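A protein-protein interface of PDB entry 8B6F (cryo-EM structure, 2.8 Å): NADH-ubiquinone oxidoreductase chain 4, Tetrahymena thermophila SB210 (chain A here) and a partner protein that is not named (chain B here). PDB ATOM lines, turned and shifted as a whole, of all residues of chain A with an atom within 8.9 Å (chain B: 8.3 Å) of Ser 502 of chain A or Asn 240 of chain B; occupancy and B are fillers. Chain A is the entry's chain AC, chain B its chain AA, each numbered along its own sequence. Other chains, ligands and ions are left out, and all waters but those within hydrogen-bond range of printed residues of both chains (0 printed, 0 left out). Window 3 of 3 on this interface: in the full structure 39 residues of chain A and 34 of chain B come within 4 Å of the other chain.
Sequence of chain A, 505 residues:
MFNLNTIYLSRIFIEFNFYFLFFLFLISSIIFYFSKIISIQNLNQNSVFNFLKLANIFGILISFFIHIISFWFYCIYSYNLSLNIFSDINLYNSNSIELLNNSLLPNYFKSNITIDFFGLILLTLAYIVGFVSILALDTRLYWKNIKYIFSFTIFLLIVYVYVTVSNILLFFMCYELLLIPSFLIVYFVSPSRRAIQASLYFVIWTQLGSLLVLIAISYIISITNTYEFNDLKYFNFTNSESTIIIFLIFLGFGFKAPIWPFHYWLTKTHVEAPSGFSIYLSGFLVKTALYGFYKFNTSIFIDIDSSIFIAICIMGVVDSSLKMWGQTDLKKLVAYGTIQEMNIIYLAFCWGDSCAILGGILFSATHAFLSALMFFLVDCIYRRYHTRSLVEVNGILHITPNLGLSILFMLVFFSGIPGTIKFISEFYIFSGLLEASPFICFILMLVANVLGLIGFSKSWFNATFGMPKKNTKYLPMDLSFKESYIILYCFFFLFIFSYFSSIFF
Of the 11 printed residues of chain B, 6 touch a printed residue of chain A. Printed residues of chain B that touch a printed residue of chain A: Met 236, Tyr 237, Leu 238, Ser 239, Asn 240 and Phe 358. Of the 21 printed residues of chain A, 9 touch a printed residue of chain B. Printed residues of chain A that touch a printed residue of chain B: Leu 358, Ile 424, Phe 427, Tyr 428, Phe 497, Ser 498, Phe 500, Ser 502 and Phe 505. Among the printed residues, 18 pairs touch across the chains. Among the printed residues, no Asp or Glu carboxylate lies within 4 Å of a Lys or Arg side-chain nitrogen of the other chain.
N of Val 244 of chain B is in hydrogen-bond range of O of Met 236 of chain B (2.8 Å). The side-chain hydroxyl of Tyr 428 of chain A is in hydrogen-bond range of the chain-end carboxylate of Phe 505 of chain A (2.5 Å).
Tyr 79 of chain A touches none of the printed residues of chain B. Of the printed residues of chain B, Leu 358 of chain A touches Asn 240 (3.5 Å). Of the printed residues of chain B, Phe 500 of chain A touches Tyr 237. Ser 502 of chain A touches two residues of chain B. Printed residues of chain B within 4 Å of Phe 505 of chain A: Tyr 237, Ser 239 and Asn 240. Of the printed residues of chain A, Met 236 of chain B touches Ile 424 (3.6 Å) and Ser 498 (3.97 Å). Of the printed residues of chain A, Leu 238 of chain B touches Phe 427 (3.7 Å) and Tyr 428 (3.7 Å). Ser 239 of chain B touches two residues of chain A. Of chain A, only Leu 358, Tyr 428, Ser 502 and Phe 505 come within 4 Å of Asn 240 of chain B. Gly 241 of chain B touches none of the printed residues of chain A. The nearest residue of chain B that does not touch Ser 502 of chain A is Phe 242 of chain B (4.1 Å). The nearest printed residue of chain B that does not touch Phe 500 of chain A is Arg 243 of chain B (5.9 Å).
O of Phe 497 of chain A lies within hydrogen-bond range of OH of Tyr 237 of chain B, at 3.5 Å. O of Ser 239 of chain B lies within hydrogen-bond range of OH of Tyr 428 of chain A (2.5 Å). OD1 of Asn 240 of chain B sits close to O of Phe 505 of chain A, 3.4 Å away. OXT of Phe 505 of chain A sits close to O of Ser 239 of chain B (3.3 Å).
Among the printed residues, pairs that only touch across the chains: Leu 358 of chain A with Asn 240 of chain B (3.5 Å), Ile 424 of chain A with Met 236 of chain B (3.6 Å), Ile 424 of chain A with Tyr 237 of chain B (3.0 Å), Phe 427 of chain A with Leu 238 of chain B (3.7 Å), Phe 427 of chain A with Phe 358 of chain B (3.6 Å), Tyr 428 of chain A with Tyr 237 of chain B (3.6 Å), Tyr 428 of chain A with Leu 238 of chain B (3.7 Å), Tyr 428 of chain A with Asn 240 of chain B (3.9 Å), Ser 498 of chain A with Met 236 of chain B (3.97 Å), Ser 498 of chain A with Tyr 237 of chain B (3.0 Å), Phe 500 of chain A with Tyr 237 of chain B (3.5 Å), Ser 502 of chain A with Tyr 237 of chain B (3.4 Å), Ser 502 of chain A with Asn 240 of chain B (3.7 Å) and Phe 505 of chain A with Tyr 237 of chain B (3.6 Å).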
ATOM      1  N   TRP A  72     -13.735  38.221  -5.174  1.00  0.00           N
ATOM      2  CA  TRP A  72     -12.657  37.313  -4.803  1.00  0.00           C
ATOM      3  C   TRP A  72     -11.842  37.884  -3.650  1.00  0.00           C
ATOM      4  O   TRP A  72     -11.503  37.166  -2.705  1.00  0.00           O
ATOM      5  CB  TRP A  72     -11.768  37.030  -6.014  1.00  0.00           C
ATOM      6  CG  TRP A  72     -10.919  35.807  -5.857  1.00  0.00           C
ATOM      7  CD1 TRP A  72      -9.564  35.731  -5.977  1.00  0.00           C
ATOM      8  CD2 TRP A  72     -11.370  34.483  -5.547  1.00  0.00           C
ATOM      9  NE1 TRP A  72      -9.142  34.441  -5.764  1.00  0.00           N
ATOM     10  CE2 TRP A  72     -10.233  33.656  -5.498  1.00  0.00           C
ATOM     11  CE3 TRP A  72     -12.627  33.918  -5.308  1.00  0.00           C
ATOM     12  CZ2 TRP A  72     -10.314  32.294  -5.221  1.00  0.00           C
ATOM     13  CZ3 TRP A  72     -12.705  32.568  -5.033  1.00  0.00           C
ATOM     14  CH2 TRP A  72     -11.555  31.771  -4.991  1.00  0.00           C
ATOM     15  N   TYR A  79     -12.418  34.927   4.827  1.00  0.00           N
ATOM     16  CA  TYR A  79     -11.816  33.686   5.297  1.00  0.00           C
ATOM     17  C   TYR A  79     -10.679  33.963   6.271  1.00  0.00           C
ATOM     18  O   TYR A  79     -10.595  33.344   7.338  1.00  0.00           O
ATOM     19  CB  TYR A  79     -11.318  32.875   4.101  1.00  0.00           C
ATOM     20  CG  TYR A  79     -10.666  31.565   4.469  1.00  0.00           C
ATOM     21  CD1 TYR A  79     -11.420  30.488   4.909  1.00  0.00           C
ATOM     22  CD2 TYR A  79      -9.293  31.401   4.354  1.00  0.00           C
ATOM     23  CE1 TYR A  79     -10.823  29.289   5.240  1.00  0.00           C
ATOM     24  CE2 TYR A  79      -8.688  30.208   4.681  1.00  0.00           C
ATOM     25  CZ  TYR A  79      -9.458  29.156   5.122  1.00  0.00           C
ATOM     26  OH  TYR A  79      -8.856  27.962   5.448  1.00  0.00           O
ATOM     27  N   PHE A 117     -21.316  37.607   2.078  1.00  0.00           N
ATOM     28  CA  PHE A 117     -21.347  36.695   0.940  1.00  0.00           C
ATOM     29  C   PHE A 117     -22.698  36.729   0.238  1.00  0.00           C
ATOM     30  O   PHE A 117     -22.762  36.748  -0.996  1.00  0.00           O
ATOM     31  CB  PHE A 117     -21.017  35.274   1.401  1.00  0.00           C
ATOM     32  CG  PHE A 117     -21.090  34.257   0.307  1.00  0.00           C
ATOM     33  CD1 PHE A 117     -20.110  34.199  -0.666  1.00  0.00           C
ATOM     34  CD2 PHE A 117     -22.138  33.354   0.251  1.00  0.00           C
ATOM     35  CE1 PHE A 117     -20.174  33.265  -1.678  1.00  0.00           C
ATOM     36  CE2 PHE A 117     -22.207  32.417  -0.757  1.00  0.00           C
ATOM     37  CZ  PHE A 117     -21.223  32.371  -1.723  1.00  0.00           C
ATOM     38  N   SER A 354     -30.019  29.169  10.532  1.00  0.00           N
ATOM     39  CA  SER A 354     -29.487  27.815  10.496  1.00  0.00           C
ATOM     40  C   SER A 354     -28.759  27.605   9.168  1.00  0.00           C
ATOM     41  O   SER A 354     -28.595  28.524   8.363  1.00  0.00           O
ATOM     42  CB  SER A 354     -30.607  26.802  10.706  1.00  0.00           C
ATOM     43  OG  SER A 354     -31.568  26.882   9.668  1.00  0.00           O
ATOM     44  N   CYS A 355     -28.307  26.374   8.927  1.00  0.00           N
ATOM     45  CA  CYS A 355     -27.581  26.067   7.702  1.00  0.00           C
ATOM     46  C   CYS A 355     -28.465  26.119   6.465  1.00  0.00           C
ATOM     47  O   CYS A 355     -27.941  26.040   5.350  1.00  0.00           O
ATOM     48  CB  CYS A 355     -26.931  24.688   7.805  1.00  0.00           C
ATOM     49  SG  CYS A 355     -25.599  24.590   9.015  1.00  0.00           S
ATOM     50  N   ALA A 356     -29.784  26.238   6.629  1.00  0.00           N
ATOM     51  CA  ALA A 356     -30.668  26.340   5.475  1.00  0.00           C
ATOM     52  C   ALA A 356     -30.367  27.567   4.629  1.00  0.00           C
ATOM     53  O   ALA A 356     -30.737  27.600   3.451  1.00  0.00           O
ATOM     54  CB  ALA A 356     -32.126  26.383   5.931  1.00  0.00           C
ATOM     55  N   ILE A 357     -29.707  28.578   5.198  1.00  0.00           N
ATOM     56  CA  ILE A 357     -29.426  29.798   4.450  1.00  0.00           C
ATOM     57  C   ILE A 357     -28.482  29.515   3.290  1.00  0.00           C
ATOM     58  O   ILE A 357     -28.603  30.125   2.222  1.00  0.00           O
ATOM     59  CB  ILE A 357     -28.862  30.885   5.387  1.00  0.00           C
ATOM     60  CG1 ILE A 357     -27.505  30.451   5.958  1.00  0.00           C
ATOM     61  CG2 ILE A 357     -29.867  31.186   6.493  1.00  0.00           C
ATOM     62  CD1 ILE A 357     -26.908  31.410   6.976  1.00  0.00           C
ATOM     63  N   LEU A 358     -27.540  28.587   3.467  1.00  0.00           N
ATOM     64  CA  LEU A 358     -26.617  28.260   2.386  1.00  0.00           C
ATOM     65  C   LEU A 358     -27.363  27.688   1.189  1.00  0.00           C
ATOM     66  O   LEU A 358     -27.147  28.110   0.048  1.00  0.00           O
ATOM     67  CB  LEU A 358     -25.556  27.275   2.878  1.00  0.00           C
ATOM     68  CG  LEU A 358     -24.881  27.619   4.205  1.00  0.00           C
ATOM     69  CD1 LEU A 358     -23.874  26.550   4.573  1.00  0.00           C
ATOM     70  CD2 LEU A 358     -24.216  28.983   4.139  1.00  0.00           C
ATOM     71  N   GLY A 359     -28.240  26.715   1.429  1.00  0.00           N
ATOM     72  CA  GLY A 359     -29.053  26.194   0.344  1.00  0.00           C
ATOM     73  C   GLY A 359     -29.933  27.261  -0.273  1.00  0.00           C
ATOM     74  O   GLY A 359     -30.126  27.295  -1.490  1.00  0.00           O
ATOM     75  N   ILE A 424     -27.608  20.775  -6.516  1.00  0.00           N
ATOM     76  CA  ILE A 424     -26.974  20.995  -5.219  1.00  0.00           C
ATOM     77  C   ILE A 424     -27.941  21.684  -4.268  1.00  0.00           C
ATOM     78  O   ILE A 424     -28.062  21.304  -3.098  1.00  0.00           O
ATOM     79  CB  ILE A 424     -25.672  21.800  -5.379  1.00  0.00           C
ATOM     80  CG1 ILE A 424     -24.699  21.063  -6.305  1.00  0.00           C
ATOM     81  CG2 ILE A 424     -25.032  22.035  -4.015  1.00  0.00           C
ATOM     82  CD1 ILE A 424     -23.414  21.823  -6.589  1.00  0.00           C
ATOM     83  N   PHE A 427     -30.554  19.326  -3.149  1.00  0.00           N
ATOM     84  CA  PHE A 427     -29.986  18.395  -2.181  1.00  0.00           C
ATOM     85  C   PHE A 427     -29.905  19.032  -0.798  1.00  0.00           C
ATOM     86  O   PHE A 427     -30.287  18.416   0.203  1.00  0.00           O
ATOM     87  CB  PHE A 427     -28.606  17.940  -2.653  1.00  0.00           C
ATOM     88  CG  PHE A 427     -28.126  16.679  -1.998  1.00  0.00           C
ATOM     89  CD1 PHE A 427     -28.487  15.443  -2.510  1.00  0.00           C
ATOM     90  CD2 PHE A 427     -27.308  16.725  -0.884  1.00  0.00           C
ATOM     91  CE1 PHE A 427     -28.046  14.277  -1.920  1.00  0.00           C
ATOM     92  CE2 PHE A 427     -26.863  15.560  -0.288  1.00  0.00           C
ATOM     93  CZ  PHE A 427     -27.234  14.335  -0.807  1.00  0.00           C
ATOM     94  N   TYR A 428     -29.398  20.265  -0.720  1.00  0.00           N
ATOM     95  CA  TYR A 428     -29.335  20.958   0.565  1.00  0.00           C
ATOM     96  C   TYR A 428     -30.713  21.045   1.209  1.00  0.00           C
ATOM     97  O   TYR A 428     -30.900  20.652   2.364  1.00  0.00           O
ATOM     98  CB  TYR A 428     -28.773  22.368   0.375  1.00  0.00           C
ATOM     99  CG  TYR A 428     -27.273  22.503   0.484  1.00  0.00           C
ATOM    100  CD1 TYR A 428     -26.443  22.158  -0.573  1.00  0.00           C
ATOM    101  CD2 TYR A 428     -26.691  23.026   1.631  1.00  0.00           C
ATOM    102  CE1 TYR A 428     -25.075  22.303  -0.481  1.00  0.00           C
ATOM    103  CE2 TYR A 428     -25.324  23.175   1.732  1.00  0.00           C
ATOM    104  CZ  TYR A 428     -24.520  22.812   0.673  1.00  0.00           C
ATOM    105  OH  TYR A 428     -23.158  22.958   0.767  1.00  0.00           O
ATOM    106  N   PHE A 497     -20.531  26.753 -11.678  1.00  0.00           N
ATOM    107  CA  PHE A 497     -20.592  27.342 -10.348  1.00  0.00           C
ATOM    108  C   PHE A 497     -20.567  26.290  -9.251  1.00  0.00           C
ATOM    109  O   PHE A 497     -20.362  26.641  -8.084  1.00  0.00           O
ATOM    110  CB  PHE A 497     -21.839  28.214 -10.210  1.00  0.00           C
ATOM    111  CG  PHE A 497     -21.794  29.145  -9.033  1.00  0.00           C
ATOM    112  CD1 PHE A 497     -21.022  30.293  -9.078  1.00  0.00           C
ATOM    113  CD2 PHE A 497     -22.521  28.877  -7.886  1.00  0.00           C
ATOM    114  CE1 PHE A 497     -20.973  31.153  -8.001  1.00  0.00           C
ATOM    115  CE2 PHE A 497     -22.477  29.735  -6.805  1.00  0.00           C
ATOM    116  CZ  PHE A 497     -21.703  30.875  -6.863  1.00  0.00           C
ATOM    117  N   SER A 498     -20.767  25.015  -9.592  1.00  0.00           N
ATOM    118  CA  SER A 498     -20.662  23.951  -8.603  1.00  0.00           C
ATOM    119  C   SER A 498     -19.240  23.778  -8.090  1.00  0.00           C
ATOM    120  O   SER A 498     -19.040  23.121  -7.062  1.00  0.00           O
ATOM    121  CB  SER A 498     -21.157  22.634  -9.200  1.00  0.00           C
ATOM    122  OG  SER A 498     -22.523  22.720  -9.562  1.00  0.00           O
ATOM    123  N   TYR A 499     -18.251  24.336  -8.780  1.00  0.00           N
ATOM    124  CA  TYR A 499     -16.864  24.265  -8.348  1.00  0.00           C
ATOM    125  C   TYR A 499     -16.446  25.460  -7.504  1.00  0.00           C
ATOM    126  O   TYR A 499     -15.288  25.525  -7.080  1.00  0.00           O
ATOM    127  CB  TYR A 499     -15.945  24.148  -9.565  1.00  0.00           C
ATOM    128  CG  TYR A 499     -16.103  22.843 -10.305  1.00  0.00           C
ATOM    129  CD1 TYR A 499     -15.444  21.699  -9.883  1.00  0.00           C
ATOM    130  CD2 TYR A 499     -16.911  22.758 -11.430  1.00  0.00           C
ATOM    131  CE1 TYR A 499     -15.587  20.503 -10.557  1.00  0.00           C
ATOM    132  CE2 TYR A 499     -17.061  21.567 -12.111  1.00  0.00           C
ATOM    133  CZ  TYR A 499     -16.395  20.444 -11.671  1.00  0.00           C
ATOM    134  OH  TYR A 499     -16.539  19.255 -12.345  1.00  0.00           O
ATOM    135  N   PHE A 500     -17.353  26.399  -7.246  1.00  0.00           N
ATOM    136  CA  PHE A 500     -17.036  27.517  -6.374  1.00  0.00           C
ATOM    137  C   PHE A 500     -16.603  27.000  -5.008  1.00  0.00           C
ATOM    138  O   PHE A 500     -17.007  25.920  -4.571  1.00  0.00           O
ATOM    139  CB  PHE A 500     -18.249  28.439  -6.237  1.00  0.00           C
ATOM    140  CG  PHE A 500     -17.984  29.682  -5.437  1.00  0.00           C
ATOM    141  CD1 PHE A 500     -17.405  30.791  -6.028  1.00  0.00           C
ATOM    142  CD2 PHE A 500     -18.324  29.744  -4.096  1.00  0.00           C
ATOM    143  CE1 PHE A 500     -17.163  31.937  -5.296  1.00  0.00           C
ATOM    144  CE2 PHE A 500     -18.087  30.887  -3.359  1.00  0.00           C
ATOM    145  CZ  PHE A 500     -17.505  31.984  -3.960  1.00  0.00           C
ATOM    146  N   SER A 501     -15.761  27.781  -4.334  1.00  0.00           N
ATOM    147  CA  SER A 501     -15.203  27.350  -3.060  1.00  0.00           C
ATOM    148  C   SER A 501     -16.315  26.966  -2.095  1.00  0.00           C
ATOM    149  O   SER A 501     -17.280  27.712  -1.906  1.00  0.00           O
ATOM    150  CB  SER A 501     -14.339  28.461  -2.463  1.00  0.00           C
ATOM    151  OG  SER A 501     -15.086  29.652  -2.291  1.00  0.00           O
ATOM    152  N   SER A 502     -16.170  25.797  -1.479  1.00  0.00           N
ATOM    153  CA  SER A 502     -17.181  25.261  -0.578  1.00  0.00           C
ATOM    154  C   SER A 502     -17.144  25.899   0.802  1.00  0.00           C
ATOM    155  O   SER A 502     -17.995  25.576   1.638  1.00  0.00           O
ATOM    156  CB  SER A 502     -17.004  23.747  -0.446  1.00  0.00           C
ATOM    157  OG  SER A 502     -17.947  23.199   0.459  1.00  0.00           O
ATOM    158  N   ILE A 503     -16.186  26.789   1.064  1.00  0.00           N
ATOM    159  CA  ILE A 503     -16.084  27.403   2.384  1.00  0.00           C
ATOM    160  C   ILE A 503     -17.350  28.184   2.703  1.00  0.00           C
ATOM    161  O   ILE A 503     -17.871  28.119   3.823  1.00  0.00           O
ATOM    162  CB  ILE A 503     -14.834  28.300   2.460  1.00  0.00           C
ATOM    163  CG1 ILE A 503     -13.571  27.506   2.111  1.00  0.00           C
ATOM    164  CG2 ILE A 503     -14.702  28.922   3.845  1.00  0.00           C
ATOM    165  CD1 ILE A 503     -13.322  26.301   2.994  1.00  0.00           C
ATOM    166  N   PHE A 504     -17.862  28.932   1.733  1.00  0.00           N
ATOM    167  CA  PHE A 504     -19.035  29.768   1.946  1.00  0.00           C
ATOM    168  C   PHE A 504     -20.347  29.026   1.745  1.00  0.00           C
ATOM    169  O   PHE A 504     -21.405  29.575   2.070  1.00  0.00           O
ATOM    170  CB  PHE A 504     -18.980  30.978   1.011  1.00  0.00           C
ATOM    171  CG  PHE A 504     -17.704  31.757   1.117  1.00  0.00           C
ATOM    172  CD1 PHE A 504     -16.616  31.440   0.322  1.00  0.00           C
ATOM    173  CD2 PHE A 504     -17.587  32.795   2.022  1.00  0.00           C
ATOM    174  CE1 PHE A 504     -15.437  32.151   0.424  1.00  0.00           C
ATOM    175  CE2 PHE A 504     -16.412  33.508   2.130  1.00  0.00           C
ATOM    176  CZ  PHE A 504     -15.336  33.187   1.331  1.00  0.00           C
ATOM    177  N   PHE A 505     -20.307  27.802   1.228  1.00  0.00           N
ATOM    178  CA  PHE A 505     -21.509  26.994   1.068  1.00  0.00           C
ATOM    179  C   PHE A 505     -21.454  25.764   1.966  1.00  0.00           C
ATOM    180  O   PHE A 505     -20.462  25.521   2.653  1.00  0.00           O
ATOM    181  CB  PHE A 505     -21.685  26.566  -0.391  1.00  0.00           C
ATOM    182  CG  PHE A 505     -22.114  27.681  -1.300  1.00  0.00           C
ATOM    183  CD1 PHE A 505     -23.389  28.213  -1.209  1.00  0.00           C
ATOM    184  CD2 PHE A 505     -21.249  28.179  -2.261  1.00  0.00           C
ATOM    185  CE1 PHE A 505     -23.789  29.233  -2.049  1.00  0.00           C
ATOM    186  CE2 PHE A 505     -21.644  29.197  -3.103  1.00  0.00           C
ATOM    187  CZ  PHE A 505     -22.915  29.725  -2.998  1.00  0.00           C
ATOM    188  OXT PHE A 505     -22.404  24.985   2.029  1.00  0.00           O
ATOM    189  N   MET B 236     -18.688  17.991  -6.393  1.00  0.00           N
ATOM    190  CA  MET B 236     -19.585  19.029  -5.903  1.00  0.00           C
ATOM    191  C   MET B 236     -19.599  19.037  -4.384  1.00  0.00           C
ATOM    192  O   MET B 236     -19.235  18.057  -3.731  1.00  0.00           O
ATOM    193  CB  MET B 236     -21.020  18.828  -6.404  1.00  0.00           C
ATOM    194  CG  MET B 236     -21.176  18.882  -7.908  1.00  0.00           C
ATOM    195  SD  MET B 236     -22.899  18.796  -8.429  1.00  0.00           S
ATOM    196  CE  MET B 236     -23.363  17.175  -7.830  1.00  0.00           C
ATOM    197  N   TYR B 237     -20.050  20.160  -3.834  1.00  0.00           N
ATOM    198  CA  TYR B 237     -20.280  20.310  -2.404  1.00  0.00           C
ATOM    199  C   TYR B 237     -21.754  20.062  -2.112  1.00  0.00           C
ATOM    200  O   TYR B 237     -22.625  20.644  -2.764  1.00  0.00           O
ATOM    201  CB  TYR B 237     -19.866  21.704  -1.926  1.00  0.00           C
ATOM    202  CG  TYR B 237     -20.418  22.835  -2.765  1.00  0.00           C
ATOM    203  CD1 TYR B 237     -21.662  23.386  -2.493  1.00  0.00           C
ATOM    204  CD2 TYR B 237     -19.693  23.349  -3.831  1.00  0.00           C
ATOM    205  CE1 TYR B 237     -22.168  24.419  -3.259  1.00  0.00           C
ATOM    206  CE2 TYR B 237     -20.190  24.381  -4.602  1.00  0.00           C
ATOM    207  CZ  TYR B 237     -21.427  24.909  -4.311  1.00  0.00           C
ATOM    208  OH  TYR B 237     -21.923  25.937  -5.078  1.00  0.00           O
ATOM    209  N   LEU B 238     -22.029  19.191  -1.140  1.00  0.00           N
ATOM    210  CA  LEU B 238     -23.393  18.784  -0.830  1.00  0.00           C
ATOM    211  C   LEU B 238     -23.777  19.050   0.620  1.00  0.00           C
ATOM    212  O   LEU B 238     -24.824  18.568   1.070  1.00  0.00           O
ATOM    213  CB  LEU B 238     -23.583  17.300  -1.163  1.00  0.00           C
ATOM    214  CG  LEU B 238     -23.438  16.927  -2.643  1.00  0.00           C
ATOM    215  CD1 LEU B 238     -23.554  15.427  -2.826  1.00  0.00           C
ATOM    216  CD2 LEU B 238     -24.472  17.642  -3.500  1.00  0.00           C
ATOM    217  N   SER B 239     -22.968  19.796   1.362  1.00  0.00           N
ATOM    218  CA  SER B 239     -23.301  20.190   2.726  1.00  0.00           C
ATOM    219  C   SER B 239     -22.361  21.319   3.130  1.00  0.00           C
ATOM    220  O   SER B 239     -21.563  21.804   2.323  1.00  0.00           O
ATOM    221  CB  SER B 239     -23.216  19.002   3.689  1.00  0.00           C
ATOM    222  OG  SER B 239     -24.118  17.977   3.314  1.00  0.00           O
ATOM    223  N   ASN B 240     -22.455  21.737   4.393  1.00  0.00           N
ATOM    224  CA  ASN B 240     -21.675  22.879   4.850  1.00  0.00           C
ATOM    225  C   ASN B 240     -20.180  22.641   4.682  1.00  0.00           C
ATOM    226  O   ASN B 240     -19.423  23.595   4.465  1.00  0.00           O
ATOM    227  CB  ASN B 240     -22.009  23.185   6.309  1.00  0.00           C
ATOM    228  CG  ASN B 240     -21.383  24.473   6.791  1.00  0.00           C
ATOM    229  OD1 ASN B 240     -20.898  25.274   5.995  1.00  0.00           O
ATOM    230  ND2 ASN B 240     -21.401  24.687   8.101  1.00  0.00           N
ATOM    231  N   GLY B 241     -19.736  21.392   4.781  1.00  0.00           N
ATOM    232  CA  GLY B 241     -18.329  21.079   4.621  1.00  0.00           C
ATOM    233  C   GLY B 241     -18.085  19.777   3.888  1.00  0.00           C
ATOM    234  O   GLY B 241     -16.971  19.247   3.910  1.00  0.00           O
ATOM    235  N   PHE B 242     -19.115  19.253   3.233  1.00  0.00           N
ATOM    236  CA  PHE B 242     -19.029  18.000   2.502  1.00  0.00           C
ATOM    237  C   PHE B 242     -18.776  18.272   1.027  1.00  0.00           C
ATOM    238  O   PHE B 242     -19.135  19.327   0.501  1.00  0.00           O
ATOM    239  CB  PHE B 242     -20.316  17.189   2.668  1.00  0.00           C
ATOM    240  CG  PHE B 242     -20.222  15.785   2.154  1.00  0.00           C
ATOM    241  CD1 PHE B 242     -19.592  14.805   2.899  1.00  0.00           C
ATOM    242  CD2 PHE B 242     -20.780  15.439   0.936  1.00  0.00           C
ATOM    243  CE1 PHE B 242     -19.509  13.510   2.434  1.00  0.00           C
ATOM    244  CE2 PHE B 242     -20.703  14.145   0.464  1.00  0.00           C
ATOM    245  CZ  PHE B 242     -20.066  13.179   1.215  1.00  0.00           C
ATOM    246  N   ARG B 243     -18.146  17.307   0.361  1.00  0.00           N
ATOM    247  CA  ARG B 243     -17.864  17.436  -1.065  1.00  0.00           C
ATOM    248  C   ARG B 243     -17.693  16.037  -1.639  1.00  0.00           C
ATOM    249  O   ARG B 243     -16.730  15.344  -1.295  1.00  0.00           O
ATOM    250  CB  ARG B 243     -16.624  18.287  -1.294  1.00  0.00           C
ATOM    251  CG  ARG B 243     -16.494  18.811  -2.712  1.00  0.00           C
ATOM    252  CD  ARG B 243     -15.263  19.678  -2.870  1.00  0.00           C
ATOM    253  NE  ARG B 243     -15.095  20.125  -4.247  1.00  0.00           N
ATOM    254  CZ  ARG B 243     -14.002  20.711  -4.716  1.00  0.00           C
ATOM    255  NH1 ARG B 243     -12.952  20.933  -3.944  1.00  0.00           N
ATOM    256  NH2 ARG B 243     -13.958  21.071  -5.996  1.00  0.00           N
ATOM    257  N   VAL B 244     -18.614  15.631  -2.504  1.00  0.00           N
ATOM    258  CA  VAL B 244     -18.614  14.290  -3.075  1.00  0.00           C
ATOM    259  C   VAL B 244     -17.733  14.278  -4.315  1.00  0.00           C
ATOM    260  O   VAL B 244     -17.814  15.179  -5.157  1.00  0.00           O
ATOM    261  CB  VAL B 244     -20.046  13.835  -3.406  1.00  0.00           C
ATOM    262  CG1 VAL B 244     -20.625  14.647  -4.561  1.00  0.00           C
ATOM    263  CG2 VAL B 244     -20.071  12.352  -3.729  1.00  0.00           C
ATOM    264  N   PHE B 358     -28.258   9.508   3.158  1.00  0.00           N
ATOM    265  CA  PHE B 358     -27.338  10.568   3.557  1.00  0.00           C
ATOM    266  C   PHE B 358     -27.675  11.099   4.945  1.00  0.00           C
ATOM    267  O   PHE B 358     -26.777  11.367   5.749  1.00  0.00           O
ATOM    268  CB  PHE B 358     -27.370  11.693   2.522  1.00  0.00           C
ATOM    269  CG  PHE B 358     -26.251  12.683   2.666  1.00  0.00           C
ATOM    270  CD1 PHE B 358     -24.939  12.288   2.485  1.00  0.00           C
ATOM    271  CD2 PHE B 358     -26.512  14.011   2.954  1.00  0.00           C
ATOM    272  CE1 PHE B 358     -23.905  13.191   2.606  1.00  0.00           C
ATOM    273  CE2 PHE B 358     -25.481  14.921   3.076  1.00  0.00           C
ATOM    274  CZ  PHE B 358     -24.177  14.510   2.901  1.00  0.00           C
ATOM    275  N   TYR B 362     -23.621   9.958   7.193  1.00  0.00           N
ATOM    276  CA  TYR B 362     -23.101  11.155   6.537  1.00  0.00           C
ATOM    277  C   TYR B 362     -22.102  10.763   5.446  1.00  0.00           C
ATOM    278  O   TYR B 362     -20.950  11.192   5.420  1.00  0.00           O
ATOM    279  CB  TYR B 362     -22.471  12.067   7.581  1.00  0.00           C
ATOM    280  CG  TYR B 362     -22.114  13.450   7.098  1.00  0.00           C
ATOM    281  CD1 TYR B 362     -23.025  14.225   6.396  1.00  0.00           C
ATOM    282  CD2 TYR B 362     -20.875  14.000   7.391  1.00  0.00           C
ATOM    283  CE1 TYR B 362     -22.700  15.496   5.973  1.00  0.00           C
ATOM    284  CE2 TYR B 362     -20.541  15.266   6.971  1.00  0.00           C
ATOM    285  CZ  TYR B 362     -21.457  16.011   6.264  1.00  0.00           C
ATOM    286  OH  TYR B 362     -21.124  17.278   5.853  1.00  0.00           O
